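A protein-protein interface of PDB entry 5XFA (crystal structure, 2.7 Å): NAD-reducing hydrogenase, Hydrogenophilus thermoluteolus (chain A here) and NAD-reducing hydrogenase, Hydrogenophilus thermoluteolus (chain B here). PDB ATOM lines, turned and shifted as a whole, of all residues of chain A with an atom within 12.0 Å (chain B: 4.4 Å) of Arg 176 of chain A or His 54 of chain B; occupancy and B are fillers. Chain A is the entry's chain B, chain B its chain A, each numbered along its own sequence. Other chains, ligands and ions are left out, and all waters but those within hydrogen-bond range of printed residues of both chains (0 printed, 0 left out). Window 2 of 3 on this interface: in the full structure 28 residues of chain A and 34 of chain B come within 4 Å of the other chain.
NH1 of Arg 176 of chain A sits close to O of Phe 52 of chain B, at 3.4 Å. The backbone carbonyl oxygen (O) of Gly 312 of chain B sits at hydrogen-bond distance from the guanidinium group (NH1) of Arg 176 of chain A (2.7 Å). O of His 476 of chain B sits at hydrogen-bond distance from NE of Arg 176 of chain A (3.4 Å). OE1 of Glu 477 of chain B is in salt-bridge range of NH2 of Arg 176 of chain A (3.8 Å). The backbone carbonyl oxygen of Ser 478 of chain B sits at hydrogen-bond distance from the backbone NH of Gly 177 of chain A (3.0 Å).
NE2 of His 54 of chain B is in hydrogen-bond range of O of Trp 106 of chain B (3.1 Å). The backbone NH of His 54 of chain B is in hydrogen-bond range of the backbone carbonyl oxygen of Gly 312 of chain B (3.2 Å).
Gly 175 of chain A touches Phe 52 of chain B. His 54 of chain B touches Arg 176 of chain A (N to NH1, 3.9 Å). CB of Ala 313 of chain B touches NH1 of Arg 176 of chain A (3.5 Å). CG of Arg 176 of chain A touches O of Ser 478 of chain B, 3.2 Å away. Arg 176 of chain A touches Cys 479 of chain B. Cys 479 of chain B touches Gly 177 of chain A.
Printed residues of chain B within 4 Å of Arg 176 of chain A: Phe 52 (3.4 Å), His 54 (3.9 Å), Gly 312 (2.7 Å), Ala 313 (3.5 Å), His 476 (3.4 Å), Glu 477 (3.8 Å), Ser 478 (3.2 Å) and Cys 479 (3.99 Å). Of the printed residues of chain A, His 54 of chain B touches Arg 176. No residue of chain A comes within 4 Å of Phe 55 of chain B. No residue of chain A comes within 4 Å of Thr 58 of chain B. No residue of chain A comes within 4 Å of Thr 107 of chain B. Gly 312 of chain B touches just one residue of chain A: Arg 176. Of the printed residues of chain A, Ala 313 of chain B touches Arg 176. His 476 of chain B touches one residue of chain A. Of chain A, only Arg 176 comes within 4 Å of Glu 477 of chain B. Of the printed residues of chain B, Gly 177 of chain A touches Ser 478 (3.0 Å) and Cys 479 (3.5 Å). Of the printed residues of chain A, Cys 479 of chain B touches Arg 176 (3.99 Å) and Gly 177 (3.5 Å). The nearest printed residue of chain B that does not touch Gly 177 of chain A is Phe 52 of chain B (5.5 Å).
Among the printed residues, 11 pairs touch across the chains. Among the printed residues, Asp or Glu carboxylates within 4 Å of a Lys or Arg side-chain nitrogen of the other chain: Arg 176 of chain A with Glu 477 of chain B (3.8 Å).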
ATOM      1  N   GLU A 100      -4.387 -11.735  10.714  1.00  0.00           N
ATOM      2  CA  GLU A 100      -5.115 -10.466  10.825  1.00  0.00           C
ATOM      3  C   GLU A 100      -5.956 -10.278  12.086  1.00  0.00           C
ATOM      4  O   GLU A 100      -5.999  -9.179  12.616  1.00  0.00           O
ATOM      5  CB  GLU A 100      -6.049 -10.323   9.609  1.00  0.00           C
ATOM      6  CG  GLU A 100      -7.039  -9.167   9.668  1.00  0.00           C
ATOM      7  CD  GLU A 100      -7.902  -9.028   8.412  1.00  0.00           C
ATOM      8  OE1 GLU A 100      -8.073 -10.033   7.661  1.00  0.00           O
ATOM      9  OE2 GLU A 100      -8.434  -7.898   8.204  1.00  0.00           O
ATOM     10  N   PHE A 133      -1.458  -9.413  13.988  1.00  0.00           N
ATOM     11  CA  PHE A 133      -1.748  -7.978  13.983  1.00  0.00           C
ATOM     12  C   PHE A 133      -2.278  -7.511  15.343  1.00  0.00           C
ATOM     13  O   PHE A 133      -2.293  -6.306  15.626  1.00  0.00           O
ATOM     14  CB  PHE A 133      -2.764  -7.644  12.886  1.00  0.00           C
ATOM     15  CG  PHE A 133      -2.193  -7.673  11.496  1.00  0.00           C
ATOM     16  CD1 PHE A 133      -1.398  -8.736  11.061  1.00  0.00           C
ATOM     17  CD2 PHE A 133      -2.474  -6.659  10.609  1.00  0.00           C
ATOM     18  CE1 PHE A 133      -0.886  -8.764   9.780  1.00  0.00           C
ATOM     19  CE2 PHE A 133      -1.971  -6.688   9.331  1.00  0.00           C
ATOM     20  CZ  PHE A 133      -1.174  -7.742   8.914  1.00  0.00           C
ATOM     21  N   PRO A 135      -5.177  -6.875  16.617  1.00  0.00           N
ATOM     22  CA  PRO A 135      -6.078  -5.724  16.597  1.00  0.00           C
ATOM     23  C   PRO A 135      -6.748  -5.523  17.946  1.00  0.00           C
ATOM     24  O   PRO A 135      -6.739  -6.437  18.781  1.00  0.00           O
ATOM     25  CB  PRO A 135      -7.115  -6.101  15.547  1.00  0.00           C
ATOM     26  CG  PRO A 135      -7.059  -7.580  15.450  1.00  0.00           C
ATOM     27  CD  PRO A 135      -5.618  -7.925  15.684  1.00  0.00           C
ATOM     28  N   ARG A 137     -10.053  -4.027  18.779  1.00  0.00           N
ATOM     29  CA  ARG A 137     -11.414  -3.536  18.607  1.00  0.00           C
ATOM     30  C   ARG A 137     -12.252  -3.961  19.780  1.00  0.00           C
ATOM     31  O   ARG A 137     -11.980  -4.976  20.418  1.00  0.00           O
ATOM     32  CB  ARG A 137     -12.038  -4.104  17.345  1.00  0.00           C
ATOM     33  CG  ARG A 137     -11.393  -3.624  16.068  1.00  0.00           C
ATOM     34  CD  ARG A 137     -10.927  -4.805  15.233  1.00  0.00           C
ATOM     35  NE  ARG A 137     -11.264  -4.644  13.833  1.00  0.00           N
ATOM     36  CZ  ARG A 137     -10.895  -5.487  12.881  1.00  0.00           C
ATOM     37  NH1 ARG A 137     -10.152  -6.548  13.174  1.00  0.00           N
ATOM     38  NH2 ARG A 137     -11.275  -5.259  11.624  1.00  0.00           N
ATOM     39  N   LEU A 155     -14.942  -9.970   7.555  1.00  0.00           N
ATOM     40  CA  LEU A 155     -15.502  -9.068   6.570  1.00  0.00           C
ATOM     41  C   LEU A 155     -16.005  -9.818   5.343  1.00  0.00           C
ATOM     42  O   LEU A 155     -15.706  -9.438   4.211  1.00  0.00           O
ATOM     43  CB  LEU A 155     -14.464  -8.030   6.158  1.00  0.00           C
ATOM     44  CG  LEU A 155     -13.891  -7.268   7.349  1.00  0.00           C
ATOM     45  CD1 LEU A 155     -12.525  -6.670   7.029  1.00  0.00           C
ATOM     46  CD2 LEU A 155     -14.879  -6.188   7.799  1.00  0.00           C
ATOM     47  N   VAL A 172     -23.040  -2.426   8.546  1.00  0.00           N
ATOM     48  CA  VAL A 172     -22.298  -1.884   7.419  1.00  0.00           C
ATOM     49  C   VAL A 172     -20.824  -1.997   7.700  1.00  0.00           C
ATOM     50  O   VAL A 172     -20.402  -1.900   8.830  1.00  0.00           O
ATOM     51  CB  VAL A 172     -22.651  -0.403   7.146  1.00  0.00           C
ATOM     52  CG1 VAL A 172     -22.193   0.492   8.298  1.00  0.00           C
ATOM     53  CG2 VAL A 172     -22.048   0.065   5.825  1.00  0.00           C
ATOM     54  N   ILE A 173     -20.043  -2.234   6.663  1.00  0.00           N
ATOM     55  CA  ILE A 173     -18.595  -2.260   6.801  1.00  0.00           C
ATOM     56  C   ILE A 173     -18.061  -0.872   6.473  1.00  0.00           C
ATOM     57  O   ILE A 173     -18.330  -0.334   5.406  1.00  0.00           O
ATOM     58  CB  ILE A 173     -17.968  -3.346   5.894  1.00  0.00           C
ATOM     59  CG1 ILE A 173     -18.433  -4.741   6.354  1.00  0.00           C
ATOM     60  CG2 ILE A 173     -16.451  -3.260   5.926  1.00  0.00           C
ATOM     61  CD1 ILE A 173     -18.303  -5.843   5.321  1.00  0.00           C
ATOM     62  N   GLY A 174     -17.313  -0.293   7.393  1.00  0.00           N
ATOM     63  CA  GLY A 174     -16.738   1.028   7.202  1.00  0.00           C
ATOM     64  C   GLY A 174     -15.239   1.045   7.441  1.00  0.00           C
ATOM     65  O   GLY A 174     -14.662   0.058   7.913  1.00  0.00           O
ATOM     66  N   GLY A 175     -14.620   2.186   7.139  1.00  0.00           N
ATOM     67  CA  GLY A 175     -13.171   2.353   7.220  1.00  0.00           C
ATOM     68  C   GLY A 175     -12.516   2.027   5.896  1.00  0.00           C
ATOM     69  O   GLY A 175     -13.163   1.543   4.962  1.00  0.00           O
ATOM     70  N   ARG A 176     -11.226   2.316   5.804  1.00  0.00           N
ATOM     71  CA  ARG A 176     -10.434   1.955   4.641  1.00  0.00           C
ATOM     72  C   ARG A 176      -9.352   0.974   5.089  1.00  0.00           C
ATOM     73  O   ARG A 176      -9.049   0.883   6.266  1.00  0.00           O
ATOM     74  CB  ARG A 176      -9.817   3.206   4.007  1.00  0.00           C
ATOM     75  CG  ARG A 176      -9.329   3.015   2.574  1.00  0.00           C
ATOM     76  CD  ARG A 176      -9.154   4.339   1.844  1.00  0.00           C
ATOM     77  NE  ARG A 176      -7.954   5.053   2.294  1.00  0.00           N
ATOM     78  CZ  ARG A 176      -7.666   6.323   2.010  1.00  0.00           C
ATOM     79  NH1 ARG A 176      -8.500   7.051   1.269  1.00  0.00           N
ATOM     80  NH2 ARG A 176      -6.545   6.876   2.474  1.00  0.00           N
ATOM     81  N   GLY A 177      -8.803   0.216   4.142  1.00  0.00           N
ATOM     82  CA  GLY A 177      -7.620  -0.606   4.380  1.00  0.00           C
ATOM     83  C   GLY A 177      -7.794  -1.548   5.534  1.00  0.00           C
ATOM     84  O   GLY A 177      -8.899  -1.964   5.830  1.00  0.00           O
ATOM     85  N   ILE A 178      -6.692  -1.856   6.204  1.00  0.00           N
ATOM     86  CA  ILE A 178      -6.698  -2.719   7.395  1.00  0.00           C
ATOM     87  C   ILE A 178      -7.579  -2.164   8.545  1.00  0.00           C
ATOM     88  O   ILE A 178      -7.919  -2.898   9.464  1.00  0.00           O
ATOM     89  CB  ILE A 178      -5.258  -2.943   7.908  1.00  0.00           C
ATOM     90  CG1 ILE A 178      -5.162  -4.161   8.818  1.00  0.00           C
ATOM     91  CG2 ILE A 178      -4.735  -1.705   8.617  1.00  0.00           C
ATOM     92  CD1 ILE A 178      -5.279  -5.484   8.091  1.00  0.00           C
ATOM     93  N   ALA A 179      -7.963  -0.883   8.479  1.00  0.00           N
ATOM     94  CA  ALA A 179      -8.903  -0.299   9.451  1.00  0.00           C
ATOM     95  C   ALA A 179     -10.348  -0.758   9.246  1.00  0.00           C
ATOM     96  O   ALA A 179     -11.220  -0.518  10.087  1.00  0.00           O
ATOM     97  CB  ALA A 179      -8.836   1.220   9.413  1.00  0.00           C
ATOM     98  N   SER A 180     -10.607  -1.382   8.111  1.00  0.00           N
ATOM     99  CA  SER A 180     -11.937  -1.817   7.767  1.00  0.00           C
ATOM    100  C   SER A 180     -12.492  -2.723   8.885  1.00  0.00           C
ATOM    101  O   SER A 180     -11.826  -3.673   9.300  1.00  0.00           O
ATOM    102  CB  SER A 180     -11.923  -2.459   6.354  1.00  0.00           C
ATOM    103  OG  SER A 180     -13.120  -3.150   6.090  1.00  0.00           O
ATOM    104  N   ARG A 181     -13.689  -2.393   9.385  1.00  0.00           N
ATOM    105  CA  ARG A 181     -14.364  -3.178  10.422  1.00  0.00           C
ATOM    106  C   ARG A 181     -15.864  -3.155  10.263  1.00  0.00           C
ATOM    107  O   ARG A 181     -16.404  -2.244   9.626  1.00  0.00           O
ATOM    108  CB  ARG A 181     -14.011  -2.625  11.792  1.00  0.00           C
ATOM    109  CG  ARG A 181     -14.506  -1.210  12.078  1.00  0.00           C
ATOM    110  CD  ARG A 181     -14.530  -0.970  13.584  1.00  0.00           C
ATOM    111  NE  ARG A 181     -15.499  -1.860  14.247  1.00  0.00           N
ATOM    112  CZ  ARG A 181     -15.540  -2.133  15.554  1.00  0.00           C
ATOM    113  NH1 ARG A 181     -14.654  -1.590  16.394  1.00  0.00           N
ATOM    114  NH2 ARG A 181     -16.478  -2.959  16.025  1.00  0.00           N
ATOM    115  N   LEU A 182     -16.548  -4.121  10.867  1.00  0.00           N
ATOM    116  CA  LEU A 182     -18.024  -4.118  10.866  1.00  0.00           C
ATOM    117  C   LEU A 182     -18.588  -3.093  11.845  1.00  0.00           C
ATOM    118  O   LEU A 182     -18.184  -3.070  13.005  1.00  0.00           O
ATOM    119  CB  LEU A 182     -18.567  -5.480  11.241  1.00  0.00           C
ATOM    120  CG  LEU A 182     -20.092  -5.570  11.241  1.00  0.00           C
ATOM    121  CD1 LEU A 182     -20.629  -5.788   9.838  1.00  0.00           C
ATOM    122  CD2 LEU A 182     -20.570  -6.689  12.142  1.00  0.00           C
ATOM    123  N   LEU A 183     -19.541  -2.277  11.380  1.00  0.00           N
ATOM    124  CA  LEU A 183     -20.184  -1.229  12.200  1.00  0.00           C
ATOM    125  C   LEU A 183     -21.698  -1.355  12.199  1.00  0.00           C
ATOM    126  O   LEU A 183     -22.306  -1.733  11.201  1.00  0.00           O
ATOM    127  CB  LEU A 183     -19.840   0.171  11.689  1.00  0.00           C
ATOM    128  CG  LEU A 183     -18.362   0.523  11.583  1.00  0.00           C
ATOM    129  CD1 LEU A 183     -18.203   1.875  10.922  1.00  0.00           C
ATOM    130  CD2 LEU A 183     -17.690   0.506  12.947  1.00  0.00           C
ATOM    131  N   PHE B  52     -14.278   6.473   5.049  1.00  0.00           N
ATOM    132  CA  PHE B  52     -13.421   5.904   4.019  1.00  0.00           C
ATOM    133  C   PHE B  52     -12.444   6.935   3.455  1.00  0.00           C
ATOM    134  O   PHE B  52     -11.367   6.595   3.008  1.00  0.00           O
ATOM    135  CB  PHE B  52     -14.297   5.334   2.909  1.00  0.00           C
ATOM    136  CG  PHE B  52     -13.536   4.630   1.826  1.00  0.00           C
ATOM    137  CD1 PHE B  52     -13.226   3.298   1.940  1.00  0.00           C
ATOM    138  CD2 PHE B  52     -13.143   5.304   0.673  1.00  0.00           C
ATOM    139  CE1 PHE B  52     -12.534   2.647   0.939  1.00  0.00           C
ATOM    140  CE2 PHE B  52     -12.450   4.656  -0.337  1.00  0.00           C
ATOM    141  CZ  PHE B  52     -12.149   3.322  -0.201  1.00  0.00           C
ATOM    142  N   TYR B  53     -12.826   8.195   3.491  1.00  0.00           N
ATOM    143  CA  TYR B  53     -12.063   9.237   2.847  1.00  0.00           C
ATOM    144  C   TYR B  53     -11.105   9.919   3.823  1.00  0.00           C
ATOM    145  O   TYR B  53     -11.500  10.292   4.931  1.00  0.00           O
ATOM    146  CB  TYR B  53     -13.037  10.248   2.225  1.00  0.00           C
ATOM    147  CG  TYR B  53     -13.917   9.636   1.154  1.00  0.00           C
ATOM    148  CD1 TYR B  53     -13.406   9.338  -0.111  1.00  0.00           C
ATOM    149  CD2 TYR B  53     -15.252   9.344   1.408  1.00  0.00           C
ATOM    150  CE1 TYR B  53     -14.203   8.763  -1.085  1.00  0.00           C
ATOM    151  CE2 TYR B  53     -16.060   8.776   0.443  1.00  0.00           C
ATOM    152  CZ  TYR B  53     -15.534   8.491  -0.798  1.00  0.00           C
ATOM    153  OH  TYR B  53     -16.354   7.942  -1.755  1.00  0.00           O
ATOM    154  N   HIS B  54      -9.851  10.091   3.394  1.00  0.00           N
ATOM    155  CA  HIS B  54      -8.783  10.611   4.255  1.00  0.00           C
ATOM    156  C   HIS B  54      -9.099  12.011   4.763  1.00  0.00           C
ATOM    157  O   HIS B  54      -9.059  12.278   5.972  1.00  0.00           O
ATOM    158  CB  HIS B  54      -7.446  10.598   3.490  1.00  0.00           C
ATOM    159  CG  HIS B  54      -6.266  11.080   4.287  1.00  0.00           C
ATOM    160  ND1 HIS B  54      -5.798  10.419   5.405  1.00  0.00           N
ATOM    161  CD2 HIS B  54      -5.438  12.140   4.104  1.00  0.00           C
ATOM    162  CE1 HIS B  54      -4.746  11.060   5.886  1.00  0.00           C
ATOM    163  NE2 HIS B  54      -4.507  12.107   5.117  1.00  0.00           N
ATOM    164  N   PHE B  55      -9.434  12.900   3.840  1.00  0.00           N
ATOM    165  CA  PHE B  55      -9.658  14.293   4.189  1.00  0.00           C
ATOM    166  C   PHE B  55     -10.952  14.543   4.978  1.00  0.00           C
ATOM    167  O   PHE B  55     -11.186  15.668   5.418  1.00  0.00           O
ATOM    168  CB  PHE B  55      -9.613  15.161   2.932  1.00  0.00           C
ATOM    169  CG  PHE B  55      -8.233  15.293   2.332  1.00  0.00           C
ATOM    170  CD1 PHE B  55      -7.236  16.018   2.989  1.00  0.00           C
ATOM    171  CD2 PHE B  55      -7.928  14.705   1.102  1.00  0.00           C
ATOM    172  CE1 PHE B  55      -5.966  16.141   2.435  1.00  0.00           C
ATOM    173  CE2 PHE B  55      -6.662  14.826   0.542  1.00  0.00           C
ATOM    174  CZ  PHE B  55      -5.680  15.546   1.210  1.00  0.00           C
ATOM    175  N   PHE B  56     -11.788  13.519   5.154  1.00  0.00           N
ATOM    176  CA  PHE B  56     -12.954  13.614   6.049  1.00  0.00           C
ATOM    177  C   PHE B  56     -12.690  13.108   7.465  1.00  0.00           C
ATOM    178  O   PHE B  56     -13.595  13.147   8.290  1.00  0.00           O
ATOM    179  CB  PHE B  56     -14.173  12.855   5.474  1.00  0.00           C
ATOM    180  CG  PHE B  56     -14.854  13.552   4.325  1.00  0.00           C
ATOM    181  CD1 PHE B  56     -14.876  14.937   4.220  1.00  0.00           C
ATOM    182  CD2 PHE B  56     -15.508  12.810   3.353  1.00  0.00           C
ATOM    183  CE1 PHE B  56     -15.512  15.557   3.158  1.00  0.00           C
ATOM    184  CE2 PHE B  56     -16.152  13.429   2.294  1.00  0.00           C
ATOM    185  CZ  PHE B  56     -16.155  14.805   2.199  1.00  0.00           C
ATOM    186  N   GLN B  57     -11.487  12.608   7.748  1.00  0.00           N
ATOM    187  CA  GLN B  57     -11.168  12.079   9.069  1.00  0.00           C
ATOM    188  C   GLN B  57     -10.185  12.986   9.828  1.00  0.00           C
ATOM    189  O   GLN B  57      -9.677  12.612  10.885  1.00  0.00           O
ATOM    190  CB  GLN B  57     -10.667  10.623   8.944  1.00  0.00           C
ATOM    191  CG  GLN B  57      -9.159  10.385   8.938  1.00  0.00           C
ATOM    192  CD  GLN B  57      -8.820   8.968   9.352  1.00  0.00           C
ATOM    193  OE1 GLN B  57      -7.725   8.702   9.835  1.00  0.00           O
ATOM    194  NE2 GLN B  57      -9.771   8.055   9.187  1.00  0.00           N
ATOM    195  N   THR B  58      -9.933  14.179   9.303  1.00  0.00           N
ATOM    196  CA  THR B  58      -9.002  15.116   9.944  1.00  0.00           C
ATOM    197  C   THR B  58      -9.641  15.808  11.172  1.00  0.00           C
ATOM    198  O   THR B  58     -10.728  16.379  11.037  1.00  0.00           O
ATOM    199  CB  THR B  58      -8.540  16.185   8.933  1.00  0.00           C
ATOM    200  OG1 THR B  58      -7.979  15.536   7.781  1.00  0.00           O
ATOM    201  CG2 THR B  58      -7.501  17.112   9.558  1.00  0.00           C
ATOM    202  N   HIS B  66      -1.535  19.388   6.145  1.00  0.00           N
ATOM    203  CA  HIS B  66      -1.038  18.077   5.756  1.00  0.00           C
ATOM    204  C   HIS B  66       0.269  18.237   4.982  1.00  0.00           C
ATOM    205  O   HIS B  66       0.312  18.891   3.939  1.00  0.00           O
ATOM    206  CB  HIS B  66      -2.054  17.333   4.891  1.00  0.00           C
ATOM    207  CG  HIS B  66      -3.404  17.161   5.525  1.00  0.00           C
ATOM    208  ND1 HIS B  66      -4.398  18.117   5.440  1.00  0.00           N
ATOM    209  CD2 HIS B  66      -3.939  16.124   6.214  1.00  0.00           C
ATOM    210  CE1 HIS B  66      -5.478  17.682   6.064  1.00  0.00           C
ATOM    211  NE2 HIS B  66      -5.227  16.475   6.542  1.00  0.00           N
ATOM    212  N   TRP B 106      -0.062  14.158   7.723  1.00  0.00           N
ATOM    213  CA  TRP B 106       0.478  13.769   6.436  1.00  0.00           C
ATOM    214  C   TRP B 106      -0.606  13.560   5.395  1.00  0.00           C
ATOM    215  O   TRP B 106      -1.791  13.547   5.707  1.00  0.00           O
ATOM    216  CB  TRP B 106       1.285  12.499   6.600  1.00  0.00           C
ATOM    217  CG  TRP B 106       2.554  12.698   7.338  1.00  0.00           C
ATOM    218  CD1 TRP B 106       2.786  12.403   8.640  1.00  0.00           C
ATOM    219  CD2 TRP B 106       3.787  13.227   6.816  1.00  0.00           C
ATOM    220  NE1 TRP B 106       4.085  12.710   8.969  1.00  0.00           N
ATOM    221  CE2 TRP B 106       4.721  13.216   7.869  1.00  0.00           C
ATOM    222  CE3 TRP B 106       4.191  13.709   5.566  1.00  0.00           C
ATOM    223  CZ2 TRP B 106       6.037  13.665   7.711  1.00  0.00           C
ATOM    224  CZ3 TRP B 106       5.497  14.156   5.407  1.00  0.00           C
ATOM    225  CH2 TRP B 106       6.405  14.129   6.478  1.00  0.00           C
ATOM    226  N   THR B 107      -0.174  13.397   4.153  1.00  0.00           N
ATOM    227  CA  THR B 107      -1.060  13.066   3.045  1.00  0.00           C
ATOM    228  C   THR B 107      -0.234  12.542   1.892  1.00  0.00           C
ATOM    229  O   THR B 107       0.922  12.915   1.739  1.00  0.00           O
ATOM    230  CB  THR B 107      -1.869  14.279   2.546  1.00  0.00           C
ATOM    231  OG1 THR B 107      -2.695  13.883   1.449  1.00  0.00           O
ATOM    232  CG2 THR B 107      -0.969  15.417   2.074  1.00  0.00           C
ATOM    233  N   ALA B 311     -12.447  13.397  -2.273  1.00  0.00           N
ATOM    234  CA  ALA B 311     -12.165  13.630  -0.847  1.00  0.00           C
ATOM    235  C   ALA B 311     -11.046  12.795  -0.242  1.00  0.00           C
ATOM    236  O   ALA B 311     -11.019  12.600   0.972  1.00  0.00           O
ATOM    237  CB  ALA B 311     -13.436  13.461  -0.027  1.00  0.00           C
ATOM    238  N   GLY B 312     -10.109  12.337  -1.069  1.00  0.00           N
ATOM    239  CA  GLY B 312      -8.851  11.786  -0.572  1.00  0.00           C
ATOM    240  C   GLY B 312      -8.775  10.280  -0.639  1.00  0.00           C
ATOM    241  O   GLY B 312      -8.928   9.594   0.369  1.00  0.00           O
ATOM    242  N   ALA B 313      -8.527   9.778  -1.843  1.00  0.00           N
ATOM    243  CA  ALA B 313      -8.283   8.361  -2.070  1.00  0.00           C
ATOM    244  C   ALA B 313      -7.626   8.184  -3.447  1.00  0.00           C
ATOM    245  O   ALA B 313      -8.108   8.753  -4.438  1.00  0.00           O
ATOM    246  CB  ALA B 313      -9.595   7.583  -1.988  1.00  0.00           C
ATOM    247  N   HIS B 476      -1.525   2.438   2.876  1.00  0.00           N
ATOM    248  CA  HIS B 476      -2.482   3.453   3.319  1.00  0.00           C
ATOM    249  C   HIS B 476      -3.675   3.585   2.385  1.00  0.00           C
ATOM    250  O   HIS B 476      -4.795   3.849   2.831  1.00  0.00           O
ATOM    251  CB  HIS B 476      -1.815   4.824   3.470  1.00  0.00           C
ATOM    252  CG  HIS B 476      -2.608   5.784   4.304  1.00  0.00           C
ATOM    253  ND1 HIS B 476      -3.201   6.916   3.785  1.00  0.00           N
ATOM    254  CD2 HIS B 476      -2.922   5.764   5.625  1.00  0.00           C
ATOM    255  CE1 HIS B 476      -3.835   7.559   4.754  1.00  0.00           C
ATOM    256  NE2 HIS B 476      -3.683   6.879   5.877  1.00  0.00           N
ATOM    257  N   GLU B 477      -3.447   3.390   1.096  1.00  0.00           N
ATOM    258  CA  GLU B 477      -4.455   3.720   0.116  1.00  0.00           C
ATOM    259  C   GLU B 477      -5.309   2.521  -0.302  1.00  0.00           C
ATOM    260  O   GLU B 477      -6.330   2.683  -0.972  1.00  0.00           O
ATOM    261  CB  GLU B 477      -3.794   4.396  -1.082  1.00  0.00           C
ATOM    262  CG  GLU B 477      -3.087   5.711  -0.733  1.00  0.00           C
ATOM    263  CD  GLU B 477      -4.015   6.919  -0.561  1.00  0.00           C
ATOM    264  OE1 GLU B 477      -5.154   6.901  -1.076  1.00  0.00           O
ATOM    265  OE2 GLU B 477      -3.599   7.904   0.098  1.00  0.00           O
ATOM    266  N   SER B 478      -4.926   1.329   0.129  1.00  0.00           N
ATOM    267  CA  SER B 478      -5.737   0.127  -0.108  1.00  0.00           C
ATOM    268  C   SER B 478      -7.158   0.253   0.400  1.00  0.00           C
ATOM    269  O   SER B 478      -7.371   0.709   1.514  1.00  0.00           O
ATOM    270  CB  SER B 478      -5.128  -1.086   0.587  1.00  0.00           C
ATOM    271  OG  SER B 478      -5.970  -2.210   0.412  1.00  0.00           O
ATOM    272  N   CYS B 479      -8.128  -0.195  -0.393  1.00  0.00           N
ATOM    273  CA  CYS B 479      -9.529  -0.028  -0.002  1.00  0.00           C
ATOM    274  C   CYS B 479      -9.985  -1.008   1.088  1.00  0.00           C
ATOM    275  O   CYS B 479     -11.046  -0.823   1.646  1.00  0.00           O
ATOM    276  CB  CYS B 479     -10.458  -0.077  -1.222  1.00  0.00           C
ATOM    277  SG  CYS B 479     -11.172  -1.694  -1.604  1.00  0.00           S
